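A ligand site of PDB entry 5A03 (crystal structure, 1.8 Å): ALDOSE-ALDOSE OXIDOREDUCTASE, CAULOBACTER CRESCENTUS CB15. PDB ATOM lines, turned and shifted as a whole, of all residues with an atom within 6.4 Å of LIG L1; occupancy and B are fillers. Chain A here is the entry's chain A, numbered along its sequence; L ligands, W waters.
An oxygen (O14) of LG2 L2 sits at hydrogen-bond distance from the guanidinium group (NE) of Arg 132, at 2.7 Å.
O2 of LIG L1 lies within hydrogen-bond range of NH2 of Arg 172.
The indole nitrogen (NE1) of Trp 171 lies within hydrogen-bond range of an oxygen (O1) of LG2 L2 (2.8 Å).
A nitrogen (N7) of LG2 L2 is in hydrogen-bond range of the side-chain hydroxyl (OH) of Tyr 17, at 3.3 Å.
OD2 of Asp 185 is in hydrogen-bond range of O3 of LIG L1 (2.7 Å).
The side-chain hydroxyl (OH) of Tyr 189 is in hydrogen-bond range of an oxygen (O14) of LG2 L2, at 3.0 Å.
NZ of Lys 104 lies within hydrogen-bond range of O13 of LG2 L2 (3.1 Å).
OH of Tyr 189 lies within hydrogen-bond range of O1 of LIG L1.
The side-chain carboxylate (OE1) of Glu 103 lies within hydrogen-bond range of a nitrogen (N7) of LG2 L2, 3.0 Å away.
The side-chain amino group of Lys 104 lies within hydrogen-bond range of an oxygen (O1) of LIG L1, at 2.6 Å.
O8 of LG2 L2 sits at hydrogen-bond distance from N of Tyr 17, at 3.0 Å.
An oxygen (O9) of LG2 L2 is in salt-bridge range of the guanidinium group of Arg 172, 2.8 Å away.
An oxygen (O13) of LG2 L2 sits at hydrogen-bond distance from the backbone carbonyl oxygen of Lys 104, 2.8 Å away.
An oxygen (O2) of LIG L1 sits close to an oxygen (O13) of LG2 L2 (3.5 Å).
The side-chain carboxylate (OD1) of Asp 185 lies within salt-bridge range of the guanidinium group (NE) of Arg 172 (2.7 Å).
The side-chain hydroxyl (OH) of Tyr 189 sits at hydrogen-bond distance from the guanidinium group (NH2) of Arg 132 (3.4 Å).
The side-chain amino group of Lys 104 sits at hydrogen-bond distance from the backbone carbonyl oxygen of Asp 185 (2.8 Å).
Phe 163 touches LIG L1 (CE1 to O3, 3.4 Å).
Tyr 267 touches LIG L1 (OH to C5, 3.97 Å).
Hydrophobic or aromatic side chains within 4 Å of LIG L1: Phe 163 and Tyr 189.
Within 4 Å of LIG L1: Lys 104, Phe 163, Arg 172, Asp 185, Tyr 189 and Tyr 267.
Water W3 bridges the side-chain hydroxyl of Tyr 267 (2.8 Å) and an oxygen (O4) of LIG L1 (3.1 Å).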
ATOM      1  N   TYR A  17     -24.014 -13.406  -1.958  1.00  0.00           N
ATOM      2  CA  TYR A  17     -23.863 -14.245  -0.774  1.00  0.00           C
ATOM      3  C   TYR A  17     -25.120 -14.268   0.079  1.00  0.00           C
ATOM      4  O   TYR A  17     -25.528 -15.324   0.563  1.00  0.00           O
ATOM      5  CB  TYR A  17     -22.680 -13.794   0.066  1.00  0.00           C
ATOM      6  CG  TYR A  17     -22.252 -14.842   1.084  1.00  0.00           C
ATOM      7  CD1 TYR A  17     -21.892 -16.115   0.671  1.00  0.00           C
ATOM      8  CD2 TYR A  17     -22.220 -14.550   2.438  1.00  0.00           C
ATOM      9  CE1 TYR A  17     -21.486 -17.075   1.594  1.00  0.00           C
ATOM     10  CE2 TYR A  17     -21.815 -15.474   3.352  1.00  0.00           C
ATOM     11  CZ  TYR A  17     -21.458 -16.755   2.936  1.00  0.00           C
ATOM     12  OH  TYR A  17     -21.057 -17.681   3.872  1.00  0.00           O
ATOM     13  N   GLU A 103     -19.763  -9.900   7.680  1.00  0.00           N
ATOM     14  CA  GLU A 103     -18.995 -10.776   6.788  1.00  0.00           C
ATOM     15  C   GLU A 103     -17.506 -10.433   6.842  1.00  0.00           C
ATOM     16  O   GLU A 103     -17.140  -9.344   7.264  1.00  0.00           O
ATOM     17  CB  GLU A 103     -19.510 -10.669   5.355  1.00  0.00           C
ATOM     18  CG  GLU A 103     -20.403 -11.862   4.976  1.00  0.00           C
ATOM     19  CD  GLU A 103     -19.779 -13.178   5.394  1.00  0.00           C
ATOM     20  OE1 GLU A 103     -18.564 -13.367   5.127  1.00  0.00           O
ATOM     21  OE2 GLU A 103     -20.478 -14.017   5.996  1.00  0.00           O
ATOM     22  N   LYS A 104     -16.668 -11.386   6.447  1.00  0.00           N
ATOM     23  CA  LYS A 104     -15.241 -11.122   6.230  1.00  0.00           C
ATOM     24  C   LYS A 104     -15.019 -10.415   4.873  1.00  0.00           C
ATOM     25  O   LYS A 104     -15.886 -10.458   4.010  1.00  0.00           O
ATOM     26  CB  LYS A 104     -14.422 -12.432   6.303  1.00  0.00           C
ATOM     27  CG  LYS A 104     -15.063 -13.687   5.651  1.00  0.00           C
ATOM     28  CD  LYS A 104     -15.372 -13.538   4.141  1.00  0.00           C
ATOM     29  CE  LYS A 104     -14.130 -13.226   3.302  1.00  0.00           C
ATOM     30  NZ  LYS A 104     -14.478 -12.969   1.849  1.00  0.00           N
ATOM     31  N   PRO A 105     -13.888  -9.726   4.715  1.00  0.00           N
ATOM     32  CA  PRO A 105     -12.975  -9.332   5.782  1.00  0.00           C
ATOM     33  C   PRO A 105     -13.719  -8.322   6.681  1.00  0.00           C
ATOM     34  O   PRO A 105     -14.604  -7.647   6.194  1.00  0.00           O
ATOM     35  CB  PRO A 105     -11.806  -8.686   5.028  1.00  0.00           C
ATOM     36  CG  PRO A 105     -12.435  -8.131   3.815  1.00  0.00           C
ATOM     37  CD  PRO A 105     -13.487  -9.143   3.425  1.00  0.00           C
ATOM     38  N   ARG A 132     -17.324 -18.937   8.465  1.00  0.00           N
ATOM     39  CA  ARG A 132     -18.152 -20.152   8.442  1.00  0.00           C
ATOM     40  C   ARG A 132     -17.342 -21.443   8.502  1.00  0.00           C
ATOM     41  O   ARG A 132     -17.869 -22.483   8.921  1.00  0.00           O
ATOM     42  CB  ARG A 132     -19.014 -20.151   7.172  1.00  0.00           C
ATOM     43  CG  ARG A 132     -18.215 -19.981   5.901  1.00  0.00           C
ATOM     44  CD  ARG A 132     -19.050 -20.121   4.642  1.00  0.00           C
ATOM     45  NE  ARG A 132     -18.271 -19.726   3.472  1.00  0.00           N
ATOM     46  CZ  ARG A 132     -17.385 -20.507   2.866  1.00  0.00           C
ATOM     47  NH1 ARG A 132     -17.206 -21.764   3.277  1.00  0.00           N
ATOM     48  NH2 ARG A 132     -16.675 -20.042   1.833  1.00  0.00           N
ATOM     49  N   PHE A 163      -9.209 -17.474  -6.740  1.00  0.00           N
ATOM     50  CA  PHE A 163     -10.057 -17.833  -7.853  1.00  0.00           C
ATOM     51  C   PHE A 163      -9.793 -16.856  -8.989  1.00  0.00           C
ATOM     52  O   PHE A 163      -9.249 -15.763  -8.768  1.00  0.00           O
ATOM     53  CB  PHE A 163     -11.538 -17.864  -7.448  1.00  0.00           C
ATOM     54  CG  PHE A 163     -12.120 -16.518  -7.131  1.00  0.00           C
ATOM     55  CD1 PHE A 163     -11.994 -15.969  -5.864  1.00  0.00           C
ATOM     56  CD2 PHE A 163     -12.847 -15.815  -8.088  1.00  0.00           C
ATOM     57  CE1 PHE A 163     -12.545 -14.725  -5.567  1.00  0.00           C
ATOM     58  CE2 PHE A 163     -13.405 -14.555  -7.796  1.00  0.00           C
ATOM     59  CZ  PHE A 163     -13.252 -14.016  -6.538  1.00  0.00           C
ATOM     60  N   TRP A 171     -17.126  -4.483  -7.593  1.00  0.00           N
ATOM     61  CA  TRP A 171     -16.613  -3.757  -6.430  1.00  0.00           C
ATOM     62  C   TRP A 171     -15.330  -4.367  -5.829  1.00  0.00           C
ATOM     63  O   TRP A 171     -14.526  -3.648  -5.264  1.00  0.00           O
ATOM     64  CB  TRP A 171     -17.695  -3.627  -5.328  1.00  0.00           C
ATOM     65  CG  TRP A 171     -18.090  -4.889  -4.614  1.00  0.00           C
ATOM     66  CD1 TRP A 171     -19.224  -5.639  -4.832  1.00  0.00           C
ATOM     67  CD2 TRP A 171     -17.389  -5.539  -3.536  1.00  0.00           C
ATOM     68  NE1 TRP A 171     -19.244  -6.716  -3.980  1.00  0.00           N
ATOM     69  CE2 TRP A 171     -18.136  -6.675  -3.174  1.00  0.00           C
ATOM     70  CE3 TRP A 171     -16.201  -5.270  -2.855  1.00  0.00           C
ATOM     71  CZ2 TRP A 171     -17.728  -7.544  -2.156  1.00  0.00           C
ATOM     72  CZ3 TRP A 171     -15.793  -6.139  -1.837  1.00  0.00           C
ATOM     73  CH2 TRP A 171     -16.566  -7.256  -1.506  1.00  0.00           C
ATOM     74  N   ARG A 172     -15.131  -5.684  -5.950  1.00  0.00           N
ATOM     75  CA  ARG A 172     -13.909  -6.288  -5.397  1.00  0.00           C
ATOM     76  C   ARG A 172     -12.627  -5.745  -6.039  1.00  0.00           C
ATOM     77  O   ARG A 172     -11.555  -5.833  -5.440  1.00  0.00           O
ATOM     78  CB  ARG A 172     -13.948  -7.820  -5.558  1.00  0.00           C
ATOM     79  CG  ARG A 172     -14.808  -8.525  -4.550  1.00  0.00           C
ATOM     80  CD  ARG A 172     -14.997 -10.004  -4.928  1.00  0.00           C
ATOM     81  NE  ARG A 172     -15.702 -10.724  -3.885  1.00  0.00           N
ATOM     82  CZ  ARG A 172     -17.024 -10.846  -3.817  1.00  0.00           C
ATOM     83  NH1 ARG A 172     -17.796 -10.267  -4.729  1.00  0.00           N
ATOM     84  NH2 ARG A 172     -17.584 -11.545  -2.832  1.00  0.00           N
ATOM     85  N   ASP A 185     -10.191 -10.584   0.045  1.00  0.00           N
ATOM     86  CA  ASP A 185     -11.354 -11.361  -0.348  1.00  0.00           C
ATOM     87  C   ASP A 185     -11.208 -12.863  -0.131  1.00  0.00           C
ATOM     88  O   ASP A 185     -12.105 -13.513   0.408  1.00  0.00           O
ATOM     89  CB  ASP A 185     -11.675 -11.114  -1.811  1.00  0.00           C
ATOM     90  CG  ASP A 185     -12.943 -11.794  -2.255  1.00  0.00           C
ATOM     91  OD1 ASP A 185     -14.028 -11.355  -1.815  1.00  0.00           O
ATOM     92  OD2 ASP A 185     -12.870 -12.779  -3.025  1.00  0.00           O
ATOM     93  N   ILE A 186     -10.092 -13.419  -0.574  1.00  0.00           N
ATOM     94  CA  ILE A 186      -9.960 -14.879  -0.566  1.00  0.00           C
ATOM     95  C   ILE A 186      -8.684 -15.353   0.147  1.00  0.00           C
ATOM     96  O   ILE A 186      -8.681 -16.399   0.810  1.00  0.00           O
ATOM     97  CB  ILE A 186     -10.029 -15.391  -2.029  1.00  0.00           C
ATOM     98  CG1 ILE A 186      -9.984 -16.919  -2.088  1.00  0.00           C
ATOM     99  CG2 ILE A 186      -8.973 -14.706  -2.916  1.00  0.00           C
ATOM    100  CD1 ILE A 186     -11.212 -17.582  -1.478  1.00  0.00           C
ATOM    101  N   ILE A 188      -7.548 -14.130   2.748  1.00  0.00           N
ATOM    102  CA  ILE A 188      -7.854 -14.140   4.165  1.00  0.00           C
ATOM    103  C   ILE A 188      -8.192 -15.575   4.667  1.00  0.00           C
ATOM    104  O   ILE A 188      -7.959 -15.896   5.845  1.00  0.00           O
ATOM    105  CB  ILE A 188      -9.006 -13.151   4.471  1.00  0.00           C
ATOM    106  CG1 ILE A 188      -9.182 -12.952   5.982  1.00  0.00           C
ATOM    107  CG2 ILE A 188     -10.297 -13.574   3.740  1.00  0.00           C
ATOM    108  CD1 ILE A 188     -10.117 -11.758   6.372  1.00  0.00           C
ATOM    109  N   TYR A 189      -8.715 -16.453   3.801  1.00  0.00           N
ATOM    110  CA  TYR A 189      -8.985 -17.826   4.233  1.00  0.00           C
ATOM    111  C   TYR A 189      -7.694 -18.573   4.571  1.00  0.00           C
ATOM    112  O   TYR A 189      -7.648 -19.376   5.521  1.00  0.00           O
ATOM    113  CB  TYR A 189      -9.781 -18.604   3.161  1.00  0.00           C
ATOM    114  CG  TYR A 189     -11.235 -18.194   3.061  1.00  0.00           C
ATOM    115  CD1 TYR A 189     -11.626 -17.184   2.184  1.00  0.00           C
ATOM    116  CD2 TYR A 189     -12.223 -18.835   3.807  1.00  0.00           C
ATOM    117  CE1 TYR A 189     -12.959 -16.808   2.077  1.00  0.00           C
ATOM    118  CE2 TYR A 189     -13.552 -18.465   3.719  1.00  0.00           C
ATOM    119  CZ  TYR A 189     -13.906 -17.451   2.845  1.00  0.00           C
ATOM    120  OH  TYR A 189     -15.226 -17.069   2.737  1.00  0.00           O
ATOM    121  N   TYR A 243      -5.975 -13.792  -7.401  1.00  0.00           N
ATOM    122  CA  TYR A 243      -7.150 -13.515  -8.214  1.00  0.00           C
ATOM    123  C   TYR A 243      -6.973 -14.026  -9.658  1.00  0.00           C
ATOM    124  O   TYR A 243      -7.767 -13.683 -10.526  1.00  0.00           O
ATOM    125  CB  TYR A 243      -7.446 -12.009  -8.223  1.00  0.00           C
ATOM    126  CG  TYR A 243      -8.443 -11.483  -7.202  1.00  0.00           C
ATOM    127  CD1 TYR A 243      -9.367 -12.330  -6.583  1.00  0.00           C
ATOM    128  CD2 TYR A 243      -8.467 -10.136  -6.884  1.00  0.00           C
ATOM    129  CE1 TYR A 243     -10.293 -11.814  -5.668  1.00  0.00           C
ATOM    130  CE2 TYR A 243      -9.378  -9.624  -5.984  1.00  0.00           C
ATOM    131  CZ  TYR A 243     -10.291 -10.463  -5.376  1.00  0.00           C
ATOM    132  OH  TYR A 243     -11.195  -9.931  -4.482  1.00  0.00           O
ATOM    133  N   THR A 265     -12.340 -24.762   2.079  1.00  0.00           N
ATOM    134  CA  THR A 265     -13.241 -23.748   2.638  1.00  0.00           C
ATOM    135  C   THR A 265     -14.308 -23.297   1.620  1.00  0.00           C
ATOM    136  O   THR A 265     -14.845 -22.178   1.688  1.00  0.00           O
ATOM    137  CB  THR A 265     -12.428 -22.519   3.134  1.00  0.00           C
ATOM    138  OG1 THR A 265     -11.760 -21.912   2.018  1.00  0.00           O
ATOM    139  CG2 THR A 265     -11.364 -22.961   4.166  1.00  0.00           C
ATOM    140  N   TYR A 267     -18.065 -23.746  -0.377  1.00  0.00           N
ATOM    141  CA  TYR A 267     -19.443 -23.858   0.118  1.00  0.00           C
ATOM    142  C   TYR A 267     -19.849 -25.302   0.352  1.00  0.00           C
ATOM    143  O   TYR A 267     -20.648 -25.600   1.235  1.00  0.00           O
ATOM    144  CB  TYR A 267     -20.424 -23.194  -0.870  1.00  0.00           C
ATOM    145  CG  TYR A 267     -20.183 -21.726  -1.112  1.00  0.00           C
ATOM    146  CD1 TYR A 267     -19.626 -20.910  -0.145  1.00  0.00           C
ATOM    147  CD2 TYR A 267     -20.531 -21.148  -2.328  1.00  0.00           C
ATOM    148  CE1 TYR A 267     -19.405 -19.558  -0.378  1.00  0.00           C
ATOM    149  CE2 TYR A 267     -20.328 -19.796  -2.578  1.00  0.00           C
ATOM    150  CZ  TYR A 267     -19.779 -19.012  -1.599  1.00  0.00           C
ATOM    151  OH  TYR A 267     -19.578 -17.671  -1.842  1.00  0.00           O
HETATM  152  O1  LIG L   1     -15.413 -15.264   1.012  1.00  0.00           O
HETATM  153  C1  LIG L   1     -15.670 -15.586  -0.333  1.00  0.00           C
HETATM  154  C2  LIG L   1     -15.232 -14.479  -1.260  1.00  0.00           C
HETATM  155  C3  LIG L   1     -15.731 -14.820  -2.653  1.00  0.00           C
HETATM  156  C4  LIG L   1     -15.284 -16.221  -3.033  1.00  0.00           C
HETATM  157  C5  LIG L   1     -15.631 -17.209  -1.925  1.00  0.00           C
HETATM  158  O2  LIG L   1     -15.759 -13.230  -0.838  1.00  0.00           O
HETATM  159  O3  LIG L   1     -15.237 -13.873  -3.593  1.00  0.00           O
HETATM  160  O4  LIG L   1     -15.909 -16.588  -4.243  1.00  0.00           O
HETATM  161  O5  LIG L   1     -15.062 -16.812  -0.680  1.00  0.00           O
HETATM  162  P1  LG2 L   2     -22.377  -8.700  -4.132  1.00  0.00           P
HETATM  163  O1  LG2 L   2     -21.734  -7.644  -4.972  1.00  0.00           O
HETATM  164  O2  LG2 L   2     -22.883  -9.966  -4.776  1.00  0.00           O
HETATM  165  O3  LG2 L   2     -23.639  -8.065  -3.272  1.00  0.00           O
HETATM  166  C1  LG2 L   2     -23.174  -6.945  -2.549  1.00  0.00           C
HETATM  167  C2  LG2 L   2     -24.434  -6.215  -2.068  1.00  0.00           C
HETATM  168  O4  LG2 L   2     -24.134  -5.166  -1.126  1.00  0.00           O
HETATM  169  C3  LG2 L   2     -25.106  -5.558  -3.291  1.00  0.00           C
HETATM  170  O5  LG2 L   2     -25.933  -6.470  -3.958  1.00  0.00           O
HETATM  171  C4  LG2 L   2     -26.004  -4.519  -2.595  1.00  0.00           C
HETATM  172  O6  LG2 L   2     -27.112  -5.060  -2.133  1.00  0.00           O
HETATM  173  C5  LG2 L   2     -25.094  -4.145  -1.328  1.00  0.00           C
HETATM  174  N1  LG2 L   2     -24.430  -2.858  -1.524  1.00  0.00           N
HETATM  175  C6  LG2 L   2     -24.559  -1.712  -0.742  1.00  0.00           C
HETATM  176  N2  LG2 L   2     -23.846  -0.686  -1.198  1.00  0.00           N
HETATM  177  C7  LG2 L   2     -23.213  -1.171  -2.327  1.00  0.00           C
HETATM  178  C8  LG2 L   2     -22.343  -0.575  -3.222  1.00  0.00           C
HETATM  179  N3  LG2 L   2     -21.962   0.742  -3.040  1.00  0.00           N
HETATM  180  N4  LG2 L   2     -21.834  -1.251  -4.290  1.00  0.00           N
HETATM  181  C9  LG2 L   2     -22.257  -2.562  -4.407  1.00  0.00           C
HETATM  182  N5  LG2 L   2     -23.087  -3.263  -3.631  1.00  0.00           N
HETATM  183  C10 LG2 L   2     -23.566  -2.531  -2.573  1.00  0.00           C
HETATM  184  O7  LG2 L   2     -21.141  -9.056  -3.100  1.00  0.00           O
HETATM  185  P2  LG2 L   2     -21.199 -10.512  -2.399  1.00  0.00           P
HETATM  186  O8  LG2 L   2     -22.470 -10.828  -1.727  1.00  0.00           O
HETATM  187  O9  LG2 L   2     -20.349 -11.548  -3.105  1.00  0.00           O
HETATM  188  O10 LG2 L   2     -20.126 -10.195  -1.028  1.00  0.00           O
HETATM  189  C11 LG2 L   2     -20.651  -9.255  -0.137  1.00  0.00           C
HETATM  190  C12 LG2 L   2     -19.884  -9.434   1.224  1.00  0.00           C
HETATM  191  O11 LG2 L   2     -19.918 -10.833   1.615  1.00  0.00           O
HETATM  192  C13 LG2 L   2     -18.369  -9.097   1.043  1.00  0.00           C
HETATM  193  O12 LG2 L   2     -17.886  -8.514   2.251  1.00  0.00           O
HETATM  194  C14 LG2 L   2     -17.725 -10.494   0.825  1.00  0.00           C
HETATM  195  O13 LG2 L   2     -16.402 -10.573   1.293  1.00  0.00           O
HETATM  196  C15 LG2 L   2     -18.617 -11.370   1.751  1.00  0.00           C
HETATM  197  N6  LG2 L   2     -18.674 -12.748   1.246  1.00  0.00           N
HETATM  198  C16 LG2 L   2     -18.423 -13.832   2.098  1.00  0.00           C
HETATM  199  C17 LG2 L   2     -18.518 -15.115   1.603  1.00  0.00           C
HETATM  200  C18 LG2 L   2     -18.264 -16.256   2.499  1.00  0.00           C
HETATM  201  O14 LG2 L   2     -18.159 -17.442   2.098  1.00  0.00           O
HETATM  202  N7  LG2 L   2     -18.172 -16.016   3.855  1.00  0.00           N
HETATM  203  C19 LG2 L   2     -18.897 -15.397   0.191  1.00  0.00           C
HETATM  204  C20 LG2 L   2     -19.116 -14.191  -0.616  1.00  0.00           C
HETATM  205  C21 LG2 L   2     -19.019 -12.962  -0.085  1.00  0.00           C
HETATM  206  P3  LG2 L   2     -28.557  -4.107  -2.247  1.00  0.00           P
HETATM  207  O15 LG2 L   2     -28.096  -2.812  -1.637  1.00  0.00           O
HETATM  208  O16 LG2 L   2     -28.727  -4.144  -3.732  1.00  0.00           O
HETATM  209  O17 LG2 L   2     -29.517  -4.963  -1.408  1.00  0.00           O
HETATM  210  O   HOH W   1     -15.074 -18.445  -5.955  1.00  0.00           O
HETATM  211  O   HOH W   2     -16.811 -13.707  -5.778  1.00  0.00           O
HETATM  212  O   HOH W   3     -19.047 -16.487  -4.374  1.00  0.00           O
